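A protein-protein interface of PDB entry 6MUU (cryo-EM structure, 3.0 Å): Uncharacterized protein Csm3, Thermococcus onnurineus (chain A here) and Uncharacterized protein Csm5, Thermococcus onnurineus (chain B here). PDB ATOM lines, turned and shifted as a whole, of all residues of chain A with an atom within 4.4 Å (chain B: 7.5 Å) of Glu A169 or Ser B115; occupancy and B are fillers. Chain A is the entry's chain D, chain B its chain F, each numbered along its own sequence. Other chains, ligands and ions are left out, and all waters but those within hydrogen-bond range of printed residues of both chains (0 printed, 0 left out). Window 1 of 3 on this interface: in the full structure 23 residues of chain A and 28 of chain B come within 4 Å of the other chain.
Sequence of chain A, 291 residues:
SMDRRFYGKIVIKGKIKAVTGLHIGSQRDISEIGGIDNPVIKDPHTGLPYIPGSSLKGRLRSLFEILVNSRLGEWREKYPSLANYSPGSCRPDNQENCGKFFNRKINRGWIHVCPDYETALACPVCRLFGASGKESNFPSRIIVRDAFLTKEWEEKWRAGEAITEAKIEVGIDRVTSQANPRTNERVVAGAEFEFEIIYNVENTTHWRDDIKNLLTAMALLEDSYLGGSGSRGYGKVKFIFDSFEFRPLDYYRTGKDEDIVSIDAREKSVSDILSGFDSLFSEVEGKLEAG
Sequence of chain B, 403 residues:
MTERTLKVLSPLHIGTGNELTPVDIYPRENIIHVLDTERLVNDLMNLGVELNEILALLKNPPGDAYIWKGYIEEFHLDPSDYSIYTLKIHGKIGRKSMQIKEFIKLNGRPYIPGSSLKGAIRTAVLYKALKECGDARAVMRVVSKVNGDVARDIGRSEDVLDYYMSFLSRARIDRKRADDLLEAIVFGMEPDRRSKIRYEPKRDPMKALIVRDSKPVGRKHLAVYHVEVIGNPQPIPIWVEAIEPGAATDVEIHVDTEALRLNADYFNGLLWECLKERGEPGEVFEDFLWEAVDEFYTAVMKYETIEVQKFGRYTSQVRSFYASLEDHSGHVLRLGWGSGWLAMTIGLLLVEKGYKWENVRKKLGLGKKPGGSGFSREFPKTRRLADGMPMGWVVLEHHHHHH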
ATOM      1  N   LYS A 167       7.735  -0.891   1.551  1.00  0.00           N
ATOM      2  CA  LYS A 167       8.739  -1.929   1.726  1.00  0.00           C
ATOM      3  C   LYS A 167      10.043  -1.306   2.209  1.00  0.00           C
ATOM      4  O   LYS A 167      10.481  -0.281   1.681  1.00  0.00           O
ATOM      5  CB  LYS A 167       8.951  -2.667   0.408  1.00  0.00           C
ATOM      6  CG  LYS A 167       9.927  -3.825   0.471  1.00  0.00           C
ATOM      7  CD  LYS A 167       9.363  -4.998   1.240  1.00  0.00           C
ATOM      8  CE  LYS A 167      10.350  -6.146   1.257  1.00  0.00           C
ATOM      9  NZ  LYS A 167      10.567  -6.713  -0.100  1.00  0.00           N
ATOM     10  N   ILE A 168      10.661  -1.918   3.214  1.00  0.00           N
ATOM     11  CA  ILE A 168      11.894  -1.415   3.809  1.00  0.00           C
ATOM     12  C   ILE A 168      13.015  -2.400   3.514  1.00  0.00           C
ATOM     13  O   ILE A 168      12.890  -3.596   3.798  1.00  0.00           O
ATOM     14  CB  ILE A 168      11.741  -1.191   5.323  1.00  0.00           C
ATOM     15  CG1 ILE A 168      10.662  -0.150   5.599  1.00  0.00           C
ATOM     16  CG2 ILE A 168      13.053  -0.736   5.938  1.00  0.00           C
ATOM     17  CD1 ILE A 168      10.287  -0.045   7.053  1.00  0.00           C
ATOM     18  N   GLU A 169      14.108  -1.899   2.944  1.00  0.00           N
ATOM     19  CA  GLU A 169      15.273  -2.710   2.632  1.00  0.00           C
ATOM     20  C   GLU A 169      16.510  -2.073   3.248  1.00  0.00           C
ATOM     21  O   GLU A 169      16.507  -0.897   3.616  1.00  0.00           O
ATOM     22  CB  GLU A 169      15.453  -2.870   1.122  1.00  0.00           C
ATOM     23  CG  GLU A 169      14.327  -3.642   0.456  1.00  0.00           C
ATOM     24  CD  GLU A 169      14.501  -3.771  -1.040  1.00  0.00           C
ATOM     25  OE1 GLU A 169      15.447  -3.169  -1.588  1.00  0.00           O
ATOM     26  OE2 GLU A 169      13.681  -4.469  -1.669  1.00  0.00           O
ATOM     27  N   VAL A 170      17.574  -2.870   3.355  1.00  0.00           N
ATOM     28  CA  VAL A 170      18.810  -2.491   4.040  1.00  0.00           C
ATOM     29  C   VAL A 170      19.998  -3.056   3.272  1.00  0.00           C
ATOM     30  O   VAL A 170      20.019  -4.245   2.939  1.00  0.00           O
ATOM     31  CB  VAL A 170      18.811  -2.992   5.503  1.00  0.00           C
ATOM     32  CG1 VAL A 170      20.205  -3.052   6.076  1.00  0.00           C
ATOM     33  CG2 VAL A 170      18.015  -2.060   6.367  1.00  0.00           C
ATOM     34  N   ASN A 180      22.528   0.512   6.469  1.00  0.00           N
ATOM     35  CA  ASN A 180      21.950   1.716   5.892  1.00  0.00           C
ATOM     36  C   ASN A 180      20.542   1.398   5.410  1.00  0.00           C
ATOM     37  O   ASN A 180      20.385   0.620   4.458  1.00  0.00           O
ATOM     38  CB  ASN A 180      22.812   2.226   4.741  1.00  0.00           C
ATOM     39  CG  ASN A 180      22.464   3.645   4.329  1.00  0.00           C
ATOM     40  OD1 ASN A 180      21.559   4.270   4.883  1.00  0.00           O
ATOM     41  ND2 ASN A 180      23.196   4.166   3.351  1.00  0.00           N
ATOM     42  N   PRO A 181      19.499   1.951   6.026  1.00  0.00           N
ATOM     43  CA  PRO A 181      18.132   1.576   5.660  1.00  0.00           C
ATOM     44  C   PRO A 181      17.557   2.404   4.522  1.00  0.00           C
ATOM     45  O   PRO A 181      17.946   3.546   4.273  1.00  0.00           O
ATOM     46  CB  PRO A 181      17.354   1.833   6.956  1.00  0.00           C
ATOM     47  CG  PRO A 181      18.082   2.952   7.586  1.00  0.00           C
ATOM     48  CD  PRO A 181      19.537   2.753   7.259  1.00  0.00           C
ATOM     49  N   ARG A 182      16.602   1.792   3.824  1.00  0.00           N
ATOM     50  CA  ARG A 182      15.938   2.390   2.676  1.00  0.00           C
ATOM     51  C   ARG A 182      14.474   1.988   2.687  1.00  0.00           C
ATOM     52  O   ARG A 182      14.124   0.898   3.140  1.00  0.00           O
ATOM     53  CB  ARG A 182      16.560   1.931   1.360  1.00  0.00           C
ATOM     54  CG  ARG A 182      17.963   2.424   1.090  1.00  0.00           C
ATOM     55  CD  ARG A 182      18.472   1.816  -0.185  1.00  0.00           C
ATOM     56  NE  ARG A 182      18.727   0.387  -0.029  1.00  0.00           N
ATOM     57  CZ  ARG A 182      18.017  -0.568  -0.619  1.00  0.00           C
ATOM     58  NH1 ARG A 182      18.328  -1.839  -0.423  1.00  0.00           N
ATOM     59  NH2 ARG A 182      16.993  -0.251  -1.398  1.00  0.00           N
ATOM     60  N   ARG A 232      15.035  -8.384  -7.283  1.00  0.00           N
ATOM     61  CA  ARG A 232      14.782  -8.591  -5.869  1.00  0.00           C
ATOM     62  C   ARG A 232      13.380  -9.111  -5.627  1.00  0.00           C
ATOM     63  O   ARG A 232      13.026  -9.398  -4.481  1.00  0.00           O
ATOM     64  CB  ARG A 232      14.976  -7.286  -5.087  1.00  0.00           C
ATOM     65  CG  ARG A 232      16.413  -6.901  -4.775  1.00  0.00           C
ATOM     66  CD  ARG A 232      17.104  -6.318  -5.979  1.00  0.00           C
ATOM     67  NE  ARG A 232      18.462  -5.906  -5.717  1.00  0.00           N
ATOM     68  CZ  ARG A 232      18.811  -4.673  -5.403  1.00  0.00           C
ATOM     69  NH1 ARG A 232      20.082  -4.409  -5.187  1.00  0.00           N
ATOM     70  NH2 ARG A 232      17.902  -3.712  -5.333  1.00  0.00           N
ATOM     71  N   TYR A 234      10.485  -7.509  -7.384  1.00  0.00           N
ATOM     72  CA  TYR A 234       9.449  -6.513  -7.633  1.00  0.00           C
ATOM     73  C   TYR A 234       8.809  -6.620  -9.016  1.00  0.00           C
ATOM     74  O   TYR A 234       8.176  -5.660  -9.461  1.00  0.00           O
ATOM     75  CB  TYR A 234       9.993  -5.093  -7.472  1.00  0.00           C
ATOM     76  CG  TYR A 234      10.414  -4.666  -6.083  1.00  0.00           C
ATOM     77  CD1 TYR A 234      10.149  -5.441  -4.964  1.00  0.00           C
ATOM     78  CD2 TYR A 234      11.065  -3.457  -5.899  1.00  0.00           C
ATOM     79  CE1 TYR A 234      10.551  -5.036  -3.714  1.00  0.00           C
ATOM     80  CE2 TYR A 234      11.460  -3.042  -4.658  1.00  0.00           C
ATOM     81  CZ  TYR A 234      11.204  -3.831  -3.570  1.00  0.00           C
ATOM     82  OH  TYR A 234      11.605  -3.400  -2.330  1.00  0.00           O
ATOM     83  N   ILE B 112       8.585 -14.635   2.726  1.00  0.00           N
ATOM     84  CA  ILE B 112      10.018 -14.367   2.768  1.00  0.00           C
ATOM     85  C   ILE B 112      10.340 -13.372   1.658  1.00  0.00           C
ATOM     86  O   ILE B 112      10.030 -13.650   0.491  1.00  0.00           O
ATOM     87  CB  ILE B 112      10.836 -15.650   2.600  1.00  0.00           C
ATOM     88  CG1 ILE B 112      10.553 -16.599   3.754  1.00  0.00           C
ATOM     89  CG2 ILE B 112      12.316 -15.332   2.526  1.00  0.00           C
ATOM     90  CD1 ILE B 112      11.096 -17.962   3.539  1.00  0.00           C
ATOM     91  N   PRO B 113      10.936 -12.228   1.965  1.00  0.00           N
ATOM     92  CA  PRO B 113      11.258 -11.263   0.915  1.00  0.00           C
ATOM     93  C   PRO B 113      12.450 -11.717   0.092  1.00  0.00           C
ATOM     94  O   PRO B 113      13.392 -12.332   0.597  1.00  0.00           O
ATOM     95  CB  PRO B 113      11.574  -9.986   1.698  1.00  0.00           C
ATOM     96  CG  PRO B 113      12.069 -10.473   2.988  1.00  0.00           C
ATOM     97  CD  PRO B 113      11.318 -11.735   3.297  1.00  0.00           C
ATOM     98  N   GLY B 114      12.383 -11.419  -1.206  1.00  0.00           N
ATOM     99  CA  GLY B 114      13.427 -11.854  -2.111  1.00  0.00           C
ATOM    100  C   GLY B 114      14.715 -11.087  -1.952  1.00  0.00           C
ATOM    101  O   GLY B 114      15.794 -11.636  -2.189  1.00  0.00           O
ATOM    102  N   SER B 115      14.635  -9.825  -1.535  1.00  0.00           N
ATOM    103  CA  SER B 115      15.850  -9.052  -1.326  1.00  0.00           C
ATOM    104  C   SER B 115      16.626  -9.510  -0.099  1.00  0.00           C
ATOM    105  O   SER B 115      17.820  -9.223  -0.009  1.00  0.00           O
ATOM    106  CB  SER B 115      15.519  -7.564  -1.212  1.00  0.00           C
ATOM    107  OG  SER B 115      14.742  -7.300  -0.060  1.00  0.00           O
ATOM    108  N   SER B 116      15.986 -10.235   0.820  1.00  0.00           N
ATOM    109  CA  SER B 116      16.696 -10.848   1.936  1.00  0.00           C
ATOM    110  C   SER B 116      17.414 -12.119   1.511  1.00  0.00           C
ATOM    111  O   SER B 116      18.519 -12.394   1.983  1.00  0.00           O
ATOM    112  CB  SER B 116      15.722 -11.156   3.071  1.00  0.00           C
ATOM    113  OG  SER B 116      16.379 -11.812   4.139  1.00  0.00           O
ATOM    114  N   LEU B 117      16.794 -12.909   0.636  1.00  0.00           N
ATOM    115  CA  LEU B 117      17.408 -14.148   0.177  1.00  0.00           C
ATOM    116  C   LEU B 117      18.540 -13.886  -0.804  1.00  0.00           C
ATOM    117  O   LEU B 117      19.471 -14.691  -0.892  1.00  0.00           O
ATOM    118  CB  LEU B 117      16.342 -15.050  -0.447  1.00  0.00           C
ATOM    119  CG  LEU B 117      16.622 -16.519  -0.772  1.00  0.00           C
ATOM    120  CD1 LEU B 117      15.350 -17.311  -0.565  1.00  0.00           C
ATOM    121  CD2 LEU B 117      17.103 -16.715  -2.201  1.00  0.00           C
ATOM    122  N   LYS B 118      18.483 -12.775  -1.541  1.00  0.00           N
ATOM    123  CA  LYS B 118      19.575 -12.442  -2.447  1.00  0.00           C
ATOM    124  C   LYS B 118      20.808 -11.987  -1.679  1.00  0.00           C
ATOM    125  O   LYS B 118      21.936 -12.171  -2.149  1.00  0.00           O
ATOM    126  CB  LYS B 118      19.129 -11.361  -3.429  1.00  0.00           C
ATOM    127  CG  LYS B 118      20.085 -11.111  -4.582  1.00  0.00           C
ATOM    128  CD  LYS B 118      19.559 -10.046  -5.513  1.00  0.00           C
ATOM    129  CE  LYS B 118      20.430  -9.935  -6.738  1.00  0.00           C
ATOM    130  NZ  LYS B 118      21.783  -9.472  -6.395  1.00  0.00           N
ATOM    131  N   GLY B 119      20.616 -11.415  -0.489  1.00  0.00           N
ATOM    132  CA  GLY B 119      21.746 -10.933   0.282  1.00  0.00           C
ATOM    133  C   GLY B 119      22.527 -12.029   0.966  1.00  0.00           C
ATOM    134  O   GLY B 119      23.743 -11.904   1.143  1.00  0.00           O
ATOM    135  N   ALA B 120      21.851 -13.109   1.363  1.00  0.00           N
ATOM    136  CA  ALA B 120      22.542 -14.229   1.989  1.00  0.00           C
ATOM    137  C   ALA B 120      23.422 -14.967   0.994  1.00  0.00           C
ATOM    138  O   ALA B 120      24.438 -15.554   1.383  1.00  0.00           O
ATOM    139  CB  ALA B 120      21.530 -15.190   2.609  1.00  0.00           C
ATOM    140  N   VAL B 211      15.875 -13.121  -8.118  1.00  0.00           N
ATOM    141  CA  VAL B 211      15.102 -13.898  -7.164  1.00  0.00           C
ATOM    142  C   VAL B 211      13.770 -13.195  -6.981  1.00  0.00           C
ATOM    143  O   VAL B 211      13.653 -11.983  -7.186  1.00  0.00           O
ATOM    144  CB  VAL B 211      15.831 -14.069  -5.815  1.00  0.00           C
ATOM    145  CG1 VAL B 211      17.086 -14.898  -5.988  1.00  0.00           C
ATOM    146  CG2 VAL B 211      16.192 -12.727  -5.259  1.00  0.00           C
ATOM    147  N   ARG B 212      12.751 -13.963  -6.627  1.00  0.00           N
ATOM    148  CA  ARG B 212      11.418 -13.415  -6.460  1.00  0.00           C
ATOM    149  C   ARG B 212      10.886 -13.795  -5.091  1.00  0.00           C
ATOM    150  O   ARG B 212      11.360 -14.745  -4.465  1.00  0.00           O
ATOM    151  CB  ARG B 212      10.492 -13.883  -7.589  1.00  0.00           C
ATOM    152  CG  ARG B 212      10.832 -13.183  -8.884  1.00  0.00           C
ATOM    153  CD  ARG B 212      10.135 -13.693 -10.107  1.00  0.00           C
ATOM    154  NE  ARG B 212      10.583 -12.888 -11.236  1.00  0.00           N
ATOM    155  CZ  ARG B 212      10.327 -13.148 -12.510  1.00  0.00           C
ATOM    156  NH1 ARG B 212       9.634 -14.217 -12.856  1.00  0.00           N
ATOM    157  NH2 ARG B 212      10.793 -12.342 -13.444  1.00  0.00           N
ATOM    158  N   ASP B 213       9.920 -13.011  -4.620  1.00  0.00           N
ATOM    159  CA  ASP B 213       9.360 -13.215  -3.291  1.00  0.00           C
ATOM    160  C   ASP B 213       8.609 -14.536  -3.232  1.00  0.00           C
ATOM    161  O   ASP B 213       7.902 -14.909  -4.171  1.00  0.00           O
ATOM    162  CB  ASP B 213       8.426 -12.063  -2.926  1.00  0.00           C
ATOM    163  CG  ASP B 213       9.163 -10.757  -2.717  1.00  0.00           C
ATOM    164  OD1 ASP B 213      10.337 -10.796  -2.311  1.00  0.00           O
ATOM    165  OD2 ASP B 213       8.568  -9.686  -2.954  1.00  0.00           O
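The side-chain carboxylate (OE2) of Glu A169 lies within hydrogen-bond range of the side-chain hydroxyl (OG) of Ser B115 (3.4 Å). The backbone carbonyl oxygen of Arg A232 is in hydrogen-bond range of the backbone NH of Ser B115 (3.4 Å).
The guanidinium group (NH2) of Arg A182 lies within salt-bridge range of the side-chain carboxylate (OE1) of Glu A169, 3.3 Å away. OE2 of Glu A169 sits at hydrogen-bond distance from OH of Tyr A234. The side-chain carboxylate of Asp B213 is in hydrogen-bond range of the backbone NH of Gly B114.
Glu A169 touches one residue of chain B. Of the printed residues of chain A, Ser B115 touches Glu A169 (3.4 Å) and Arg A232 (3.4 Å). Of the printed residues of chain A, Gly B114 touches Arg A232. Of the printed residues of chain A, Val B211 touches Arg A232. Of the printed residues of chain B, Lys A167 touches Pro B113. Lys B118 touches none of the printed residues of chain A. Val A170 touches none of the printed residues of chain B. The nearest printed residue of chain B that does not touch Glu A169 is Ser B116 (6.7 Å). The nearest residue of chain A that does not touch Ser B115 is Lys A167 (4.2 Å). The nearest printed residue of chain B that does not touch Arg A232 is Lys B118 (4.3 Å).
Among the printed residues, merely in contact across the chains: Arg A232 with Val B211 (3.3 Å), Arg A232 with Gly B114 (3.4 Å), Arg A232 with Asp B213 (3.7 Å) and Lys A167 with Pro B113 (3.9 Å).
Of the 9 printed residues of chain A, 3 touch a printed residue of chain B. Along chain A the printed residues that touch a printed residue of chain B span positions 167 to 232. Of the 12 printed residues of chain B, 5 touch a printed residue of chain A. Hydrophobic or aromatic side chains of chain B that line the printed part of chain A: Pro B113.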
